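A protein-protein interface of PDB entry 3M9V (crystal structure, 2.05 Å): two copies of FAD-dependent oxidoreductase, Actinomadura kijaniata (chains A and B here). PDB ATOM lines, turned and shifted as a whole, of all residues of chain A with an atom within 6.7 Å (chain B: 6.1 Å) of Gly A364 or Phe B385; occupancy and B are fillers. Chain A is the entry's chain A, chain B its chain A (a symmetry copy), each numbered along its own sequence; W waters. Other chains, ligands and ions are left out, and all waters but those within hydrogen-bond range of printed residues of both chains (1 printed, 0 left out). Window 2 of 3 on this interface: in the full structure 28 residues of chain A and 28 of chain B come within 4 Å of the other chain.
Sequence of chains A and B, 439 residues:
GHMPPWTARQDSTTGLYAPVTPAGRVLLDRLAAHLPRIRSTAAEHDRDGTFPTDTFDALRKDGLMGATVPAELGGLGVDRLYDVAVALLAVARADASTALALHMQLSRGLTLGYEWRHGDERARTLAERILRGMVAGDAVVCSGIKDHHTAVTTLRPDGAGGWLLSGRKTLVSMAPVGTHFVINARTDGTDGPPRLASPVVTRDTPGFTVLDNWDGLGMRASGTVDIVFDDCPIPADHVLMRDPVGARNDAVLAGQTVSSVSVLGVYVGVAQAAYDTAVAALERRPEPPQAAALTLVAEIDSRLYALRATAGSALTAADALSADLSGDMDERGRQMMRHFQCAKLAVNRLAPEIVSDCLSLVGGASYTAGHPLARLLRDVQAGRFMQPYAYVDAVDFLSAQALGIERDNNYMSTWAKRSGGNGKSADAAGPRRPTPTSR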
ATOM      1  N   SER A 356       9.849 -12.936   0.797  1.00  0.00           N
ATOM      2  CA  SER A 356       9.161 -11.698   1.146  1.00  0.00           C
ATOM      3  C   SER A 356       9.115 -10.695  -0.011  1.00  0.00           C
ATOM      4  O   SER A 356       8.054 -10.142  -0.328  1.00  0.00           O
ATOM      5  CB  SER A 356       9.721 -11.108   2.448  1.00  0.00           C
ATOM      6  OG  SER A 356       9.116  -9.858   2.712  1.00  0.00           O
ATOM      7  N   LEU A 359       6.322 -11.189  -2.673  1.00  0.00           N
ATOM      8  CA  LEU A 359       4.988 -10.721  -2.327  1.00  0.00           C
ATOM      9  C   LEU A 359       4.795  -9.269  -2.736  1.00  0.00           C
ATOM     10  O   LEU A 359       3.681  -8.879  -3.103  1.00  0.00           O
ATOM     11  CB  LEU A 359       4.743 -10.854  -0.819  1.00  0.00           C
ATOM     12  CG  LEU A 359       4.266 -12.254  -0.372  1.00  0.00           C
ATOM     13  CD1 LEU A 359       5.425 -13.156  -0.005  1.00  0.00           C
ATOM     14  CD2 LEU A 359       3.354 -12.247   0.828  1.00  0.00           C
ATOM     15  N   SER A 360       5.856  -8.476  -2.628  1.00  0.00           N
ATOM     16  CA  SER A 360       5.802  -7.117  -3.151  1.00  0.00           C
ATOM     17  C   SER A 360       5.582  -7.123  -4.670  1.00  0.00           C
ATOM     18  O   SER A 360       4.875  -6.248  -5.153  1.00  0.00           O
ATOM     19  CB  SER A 360       7.090  -6.352  -2.848  1.00  0.00           C
ATOM     20  OG  SER A 360       7.237  -6.280  -1.447  1.00  0.00           O
ATOM     21  N   LEU A 361       6.172  -8.048  -5.429  1.00  0.00           N
ATOM     22  CA  LEU A 361       5.914  -8.109  -6.865  1.00  0.00           C
ATOM     23  C   LEU A 361       4.479  -8.496  -7.225  1.00  0.00           C
ATOM     24  O   LEU A 361       3.885  -7.920  -8.133  1.00  0.00           O
ATOM     25  CB  LEU A 361       6.863  -9.093  -7.547  1.00  0.00           C
ATOM     26  CG  LEU A 361       8.310  -8.600  -7.448  1.00  0.00           C
ATOM     27  CD1 LEU A 361       9.330  -9.661  -7.795  1.00  0.00           C
ATOM     28  CD2 LEU A 361       8.393  -7.399  -8.390  1.00  0.00           C
ATOM     29  N   VAL A 362       3.951  -9.560  -6.633  1.00  0.00           N
ATOM     30  CA  VAL A 362       2.586  -9.971  -6.892  1.00  0.00           C
ATOM     31  C   VAL A 362       1.546  -8.996  -6.329  1.00  0.00           C
ATOM     32  O   VAL A 362       0.516  -8.825  -6.971  1.00  0.00           O
ATOM     33  CB  VAL A 362       2.344 -11.352  -6.286  1.00  0.00           C
ATOM     34  CG1 VAL A 362       0.866 -11.731  -6.459  1.00  0.00           C
ATOM     35  CG2 VAL A 362       3.293 -12.349  -6.939  1.00  0.00           C
ATOM     36  N   GLY A 363       1.793  -8.397  -5.169  1.00  0.00           N
ATOM     37  CA  GLY A 363       0.880  -7.488  -4.484  1.00  0.00           C
ATOM     38  C   GLY A 363      -0.198  -8.221  -3.694  1.00  0.00           C
ATOM     39  O   GLY A 363      -0.010  -9.398  -3.396  1.00  0.00           O
ATOM     40  N   GLY A 364      -1.336  -7.567  -3.438  1.00  0.00           N
ATOM     41  CA  GLY A 364      -2.339  -7.965  -2.447  1.00  0.00           C
ATOM     42  C   GLY A 364      -2.930  -9.359  -2.558  1.00  0.00           C
ATOM     43  O   GLY A 364      -3.238 -10.001  -1.544  1.00  0.00           O
ATOM     44  N   ALA A 365      -3.024  -9.884  -3.778  1.00  0.00           N
ATOM     45  CA  ALA A 365      -3.473 -11.272  -3.948  1.00  0.00           C
ATOM     46  C   ALA A 365      -2.613 -12.257  -3.158  1.00  0.00           C
ATOM     47  O   ALA A 365      -3.101 -13.290  -2.763  1.00  0.00           O
ATOM     48  CB  ALA A 365      -3.484 -11.684  -5.414  1.00  0.00           C
ATOM     49  N   SER A 366      -1.342 -11.968  -2.917  1.00  0.00           N
ATOM     50  CA  SER A 366      -0.484 -12.906  -2.209  1.00  0.00           C
ATOM     51  C   SER A 366      -0.769 -12.923  -0.710  1.00  0.00           C
ATOM     52  O   SER A 366      -0.236 -13.786  -0.001  1.00  0.00           O
ATOM     53  CB  SER A 366       0.971 -12.520  -2.480  1.00  0.00           C
ATOM     54  OG  SER A 366       1.260 -11.309  -1.800  1.00  0.00           O
ATOM     55  N   TYR A 367      -1.603 -12.004  -0.206  1.00  0.00           N
ATOM     56  CA  TYR A 367      -1.972 -11.957   1.214  1.00  0.00           C
ATOM     57  C   TYR A 367      -3.262 -12.714   1.593  1.00  0.00           C
ATOM     58  O   TYR A 367      -3.743 -12.644   2.732  1.00  0.00           O
ATOM     59  CB  TYR A 367      -2.017 -10.506   1.710  1.00  0.00           C
ATOM     60  CG  TYR A 367      -1.980 -10.312   3.219  1.00  0.00           C
ATOM     61  CD1 TYR A 367      -0.878 -10.686   3.989  1.00  0.00           C
ATOM     62  CD2 TYR A 367      -3.068  -9.740   3.876  1.00  0.00           C
ATOM     63  CE1 TYR A 367      -0.837 -10.507   5.377  1.00  0.00           C
ATOM     64  CE2 TYR A 367      -3.055  -9.574   5.254  1.00  0.00           C
ATOM     65  CZ  TYR A 367      -1.936  -9.954   5.988  1.00  0.00           C
ATOM     66  OH  TYR A 367      -1.939  -9.744   7.337  1.00  0.00           O
ATOM     67  N   THR A 368      -3.828 -13.479   0.661  1.00  0.00           N
ATOM     68  CA  THR A 368      -5.033 -14.218   1.018  1.00  0.00           C
ATOM     69  C   THR A 368      -4.512 -15.616   1.283  1.00  0.00           C
ATOM     70  O   THR A 368      -3.472 -16.001   0.750  1.00  0.00           O
ATOM     71  CB  THR A 368      -6.030 -14.286  -0.156  1.00  0.00           C
ATOM     72  OG1 THR A 368      -5.378 -15.022  -1.189  1.00  0.00           O
ATOM     73  CG2 THR A 368      -6.288 -12.907  -0.736  1.00  0.00           C
ATOM     74  N   LEU B 171     -12.210  -5.800  -0.221  1.00  0.00           N
ATOM     75  CA  LEU B 171     -11.360  -5.456   0.911  1.00  0.00           C
ATOM     76  C   LEU B 171     -12.027  -4.416   1.794  1.00  0.00           C
ATOM     77  O   LEU B 171     -11.402  -3.427   2.190  1.00  0.00           O
ATOM     78  CB  LEU B 171      -9.938  -5.051   0.491  1.00  0.00           C
ATOM     79  CG  LEU B 171      -9.133  -6.102  -0.283  1.00  0.00           C
ATOM     80  CD1 LEU B 171      -7.710  -5.601  -0.611  1.00  0.00           C
ATOM     81  CD2 LEU B 171      -9.048  -7.475   0.386  1.00  0.00           C
ATOM     82  N   LYS B 344       5.258   5.684   5.694  1.00  0.00           N
ATOM     83  CA  LYS B 344       4.680   4.378   5.383  1.00  0.00           C
ATOM     84  C   LYS B 344       5.694   3.382   4.842  1.00  0.00           C
ATOM     85  O   LYS B 344       5.735   2.219   5.250  1.00  0.00           O
ATOM     86  CB  LYS B 344       3.520   4.507   4.368  1.00  0.00           C
ATOM     87  CG  LYS B 344       2.769   3.190   4.150  1.00  0.00           C
ATOM     88  CD  LYS B 344       1.617   3.327   3.129  1.00  0.00           C
ATOM     89  CE  LYS B 344       0.576   2.209   3.249  1.00  0.00           C
ATOM     90  NZ  LYS B 344       1.121   1.098   2.448  1.00  0.00           N
ATOM     91  N   ASN B 348       6.599  -0.092   6.850  1.00  0.00           N
ATOM     92  CA  ASN B 348       6.429  -1.381   6.203  1.00  0.00           C
ATOM     93  C   ASN B 348       7.728  -2.173   6.038  1.00  0.00           C
ATOM     94  O   ASN B 348       7.701  -3.371   5.776  1.00  0.00           O
ATOM     95  CB  ASN B 348       5.825  -1.185   4.805  1.00  0.00           C
ATOM     96  CG  ASN B 348       4.340  -0.921   4.867  1.00  0.00           C
ATOM     97  OD1 ASN B 348       3.748  -1.230   5.888  1.00  0.00           O
ATOM     98  ND2 ASN B 348       3.731  -0.356   3.818  1.00  0.00           N
ATOM     99  N   GLN B 381       2.302  -8.041   8.064  1.00  0.00           N
ATOM    100  CA  GLN B 381       2.545  -7.907   6.626  1.00  0.00           C
ATOM    101  C   GLN B 381       1.462  -7.081   5.923  1.00  0.00           C
ATOM    102  O   GLN B 381       1.701  -6.601   4.817  1.00  0.00           O
ATOM    103  CB  GLN B 381       2.686  -9.271   5.931  1.00  0.00           C
ATOM    104  CG  GLN B 381       3.605 -10.310   6.631  1.00  0.00           C
ATOM    105  CD  GLN B 381       5.069  -9.895   6.650  1.00  0.00           C
ATOM    106  OE1 GLN B 381       5.523  -9.095   5.823  1.00  0.00           O
ATOM    107  NE2 GLN B 381       5.802 -10.383   7.644  1.00  0.00           N
ATOM    108  N   ALA B 382       0.298  -6.892   6.547  1.00  0.00           N
ATOM    109  CA  ALA B 382      -0.866  -6.349   5.844  1.00  0.00           C
ATOM    110  C   ALA B 382      -0.642  -4.911   5.354  1.00  0.00           C
ATOM    111  O   ALA B 382      -1.205  -4.537   4.339  1.00  0.00           O
ATOM    112  CB  ALA B 382      -2.058  -6.380   6.793  1.00  0.00           C
ATOM    113  N   GLY B 383       0.164  -4.095   6.034  1.00  0.00           N
ATOM    114  CA  GLY B 383       0.382  -2.683   5.669  1.00  0.00           C
ATOM    115  C   GLY B 383       0.941  -2.455   4.270  1.00  0.00           C
ATOM    116  O   GLY B 383       0.633  -1.446   3.616  1.00  0.00           O
ATOM    117  N   ARG B 384       1.726  -3.437   3.827  1.00  0.00           N
ATOM    118  CA  ARG B 384       2.423  -3.461   2.549  1.00  0.00           C
ATOM    119  C   ARG B 384       1.443  -3.431   1.388  1.00  0.00           C
ATOM    120  O   ARG B 384       1.784  -3.010   0.289  1.00  0.00           O
ATOM    121  CB  ARG B 384       3.267  -4.749   2.422  1.00  0.00           C
ATOM    122  CG  ARG B 384       4.403  -4.803   3.446  1.00  0.00           C
ATOM    123  CD  ARG B 384       5.080  -6.163   3.540  1.00  0.00           C
ATOM    124  NE  ARG B 384       5.679  -6.514   2.252  1.00  0.00           N
ATOM    125  CZ  ARG B 384       6.318  -7.662   2.073  1.00  0.00           C
ATOM    126  NH1 ARG B 384       6.391  -8.502   3.099  1.00  0.00           N
ATOM    127  NH2 ARG B 384       6.859  -7.965   0.905  1.00  0.00           N
ATOM    128  N   PHE B 385       0.231  -3.910   1.629  1.00  0.00           N
ATOM    129  CA  PHE B 385      -0.690  -4.157   0.529  1.00  0.00           C
ATOM    130  C   PHE B 385      -1.775  -3.080   0.548  1.00  0.00           C
ATOM    131  O   PHE B 385      -2.461  -2.934  -0.456  1.00  0.00           O
ATOM    132  CB  PHE B 385      -1.233  -5.599   0.557  1.00  0.00           C
ATOM    133  CG  PHE B 385      -0.123  -6.606   0.570  1.00  0.00           C
ATOM    134  CD1 PHE B 385       0.745  -6.711  -0.515  1.00  0.00           C
ATOM    135  CD2 PHE B 385       0.131  -7.341   1.720  1.00  0.00           C
ATOM    136  CE1 PHE B 385       1.813  -7.598  -0.474  1.00  0.00           C
ATOM    137  CE2 PHE B 385       1.199  -8.227   1.777  1.00  0.00           C
ATOM    138  CZ  PHE B 385       2.053  -8.345   0.675  1.00  0.00           C
ATOM    139  N   MET B 386      -1.900  -2.322   1.636  1.00  0.00           N
ATOM    140  CA  MET B 386      -2.879  -1.240   1.758  1.00  0.00           C
ATOM    141  C   MET B 386      -2.608   0.025   0.928  1.00  0.00           C
ATOM    142  O   MET B 386      -1.523   0.602   0.945  1.00  0.00           O
ATOM    143  CB  MET B 386      -3.047  -0.895   3.236  1.00  0.00           C
ATOM    144  CG  MET B 386      -3.692  -2.031   4.047  1.00  0.00           C
ATOM    145  SD  MET B 386      -3.899  -1.520   5.786  1.00  0.00           S
ATOM    146  CE  MET B 386      -2.469  -0.565   6.192  1.00  0.00           C
ATOM    147  N   GLN B 387      -3.577   0.459   0.134  1.00  0.00           N
ATOM    148  CA  GLN B 387      -3.340   1.624  -0.701  1.00  0.00           C
ATOM    149  C   GLN B 387      -3.950   2.772   0.093  1.00  0.00           C
ATOM    150  O   GLN B 387      -4.909   2.557   0.828  1.00  0.00           O
ATOM    151  CB  GLN B 387      -4.039   1.436  -2.055  1.00  0.00           C
ATOM    152  CG  GLN B 387      -3.199   0.697  -3.128  1.00  0.00           C
ATOM    153  CD  GLN B 387      -1.864   1.392  -3.420  1.00  0.00           C
ATOM    154  OE1 GLN B 387      -1.475   2.319  -2.698  1.00  0.00           O
ATOM    155  NE2 GLN B 387      -1.147   0.948  -4.454  1.00  0.00           N
ATOM    156  N   ALA B 390       0.790   0.953  -2.209  1.00  0.00           N
ATOM    157  CA  ALA B 390       1.638  -0.226  -2.088  1.00  0.00           C
ATOM    158  C   ALA B 390       3.039   0.109  -2.624  1.00  0.00           C
ATOM    159  O   ALA B 390       3.178   1.051  -3.412  1.00  0.00           O
ATOM    160  CB  ALA B 390       1.018  -1.389  -2.872  1.00  0.00           C
HETATM  161  O   HOH W   1       5.972  -4.645   0.154  1.00  0.00           O
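The backbone carbonyl oxygen of Ser A356 lies within hydrogen-bond range of the guanidinium group of Arg B384 (2.8 Å).
The side-chain hydroxyl of Ser A360 is in hydrogen-bond range of the guanidinium group of Arg B384.
The backbone carbonyl oxygen of Gly A363 sits at hydrogen-bond distance from the side-chain hydroxyl of Ser A366 (2.8 Å).
The side-chain amide oxygen of Gln B381 lies within hydrogen-bond range of the guanidinium group of Arg B384 (2.9 Å).
CB of Leu A359 touches NH2 of Arg B384 (3.97 Å).
O of Leu A359 touches CE1 of Phe B385 (3.5 Å).
CD1 of Phe B385 touches C of Gly A363, 3.6 Å away.
N of Gly A364 touches CD1 of Phe B385, at 3.7 Å.
Ser A366 touches Phe B385.
Gln B381 touches Tyr A367 (CB to CE1, 3.8 Å).
OH of Tyr A367 touches CB of Ala B382 (3.4 Å).
Tyr A367 touches Phe B385 (CB to CD2, 3.8 Å).
Val A362 touches none of the printed residues of chain B.
Gly A364 touches just one residue of chain B: Phe B385 (3.7 Å).
Printed residues of chain B within 4 Å of Ser A366: Phe B385.
Of the printed residues of chain B, Tyr A367 touches Gln B381 (3.8 Å), Ala B382 (3.4 Å) and Phe B385 (3.8 Å).
Printed residues of chain A within 4 Å of Gln B381: Tyr A367.
Of chain A, only Leu A359 (3.5 Å), Gly A363 (3.6 Å), Gly A364 (3.7 Å), Ser A366 (3.9 Å) and Tyr A367 (3.8 Å) come within 4 Å of Phe B385.
Gln B387 touches none of the printed residues of chain A.
The nearest printed residue of chain B that does not touch Ser A360 is Phe B385 (4.7 Å).
Of the 11 printed residues of chain B, 4 touch a printed residue of chain A.
Printed residues of chain B that touch a printed residue of chain A: Gln B381, Ala B382, Arg B384 and Phe B385.
Hydrophobic or aromatic side chains of chain B that line the printed part of chain A: Ala B382 and Phe B385.
Of the 11 printed residues of chain A, 7 touch a printed residue of chain B.
Hydrophobic or aromatic side chains of chain A that line the printed part of chain B: Leu A359 and Tyr A367.
Among the printed residues, 10 pairs touch across the chains.
No position is printed for both chains.
Of the 10 pairs that touch across the chains among the printed residues, none has its exchanged pair printed and touching as well.
Water W1 lies within hydrogen-bond range of OG of Ser A360 (2.6 Å) and NE of Arg B384 (2.8 Å).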
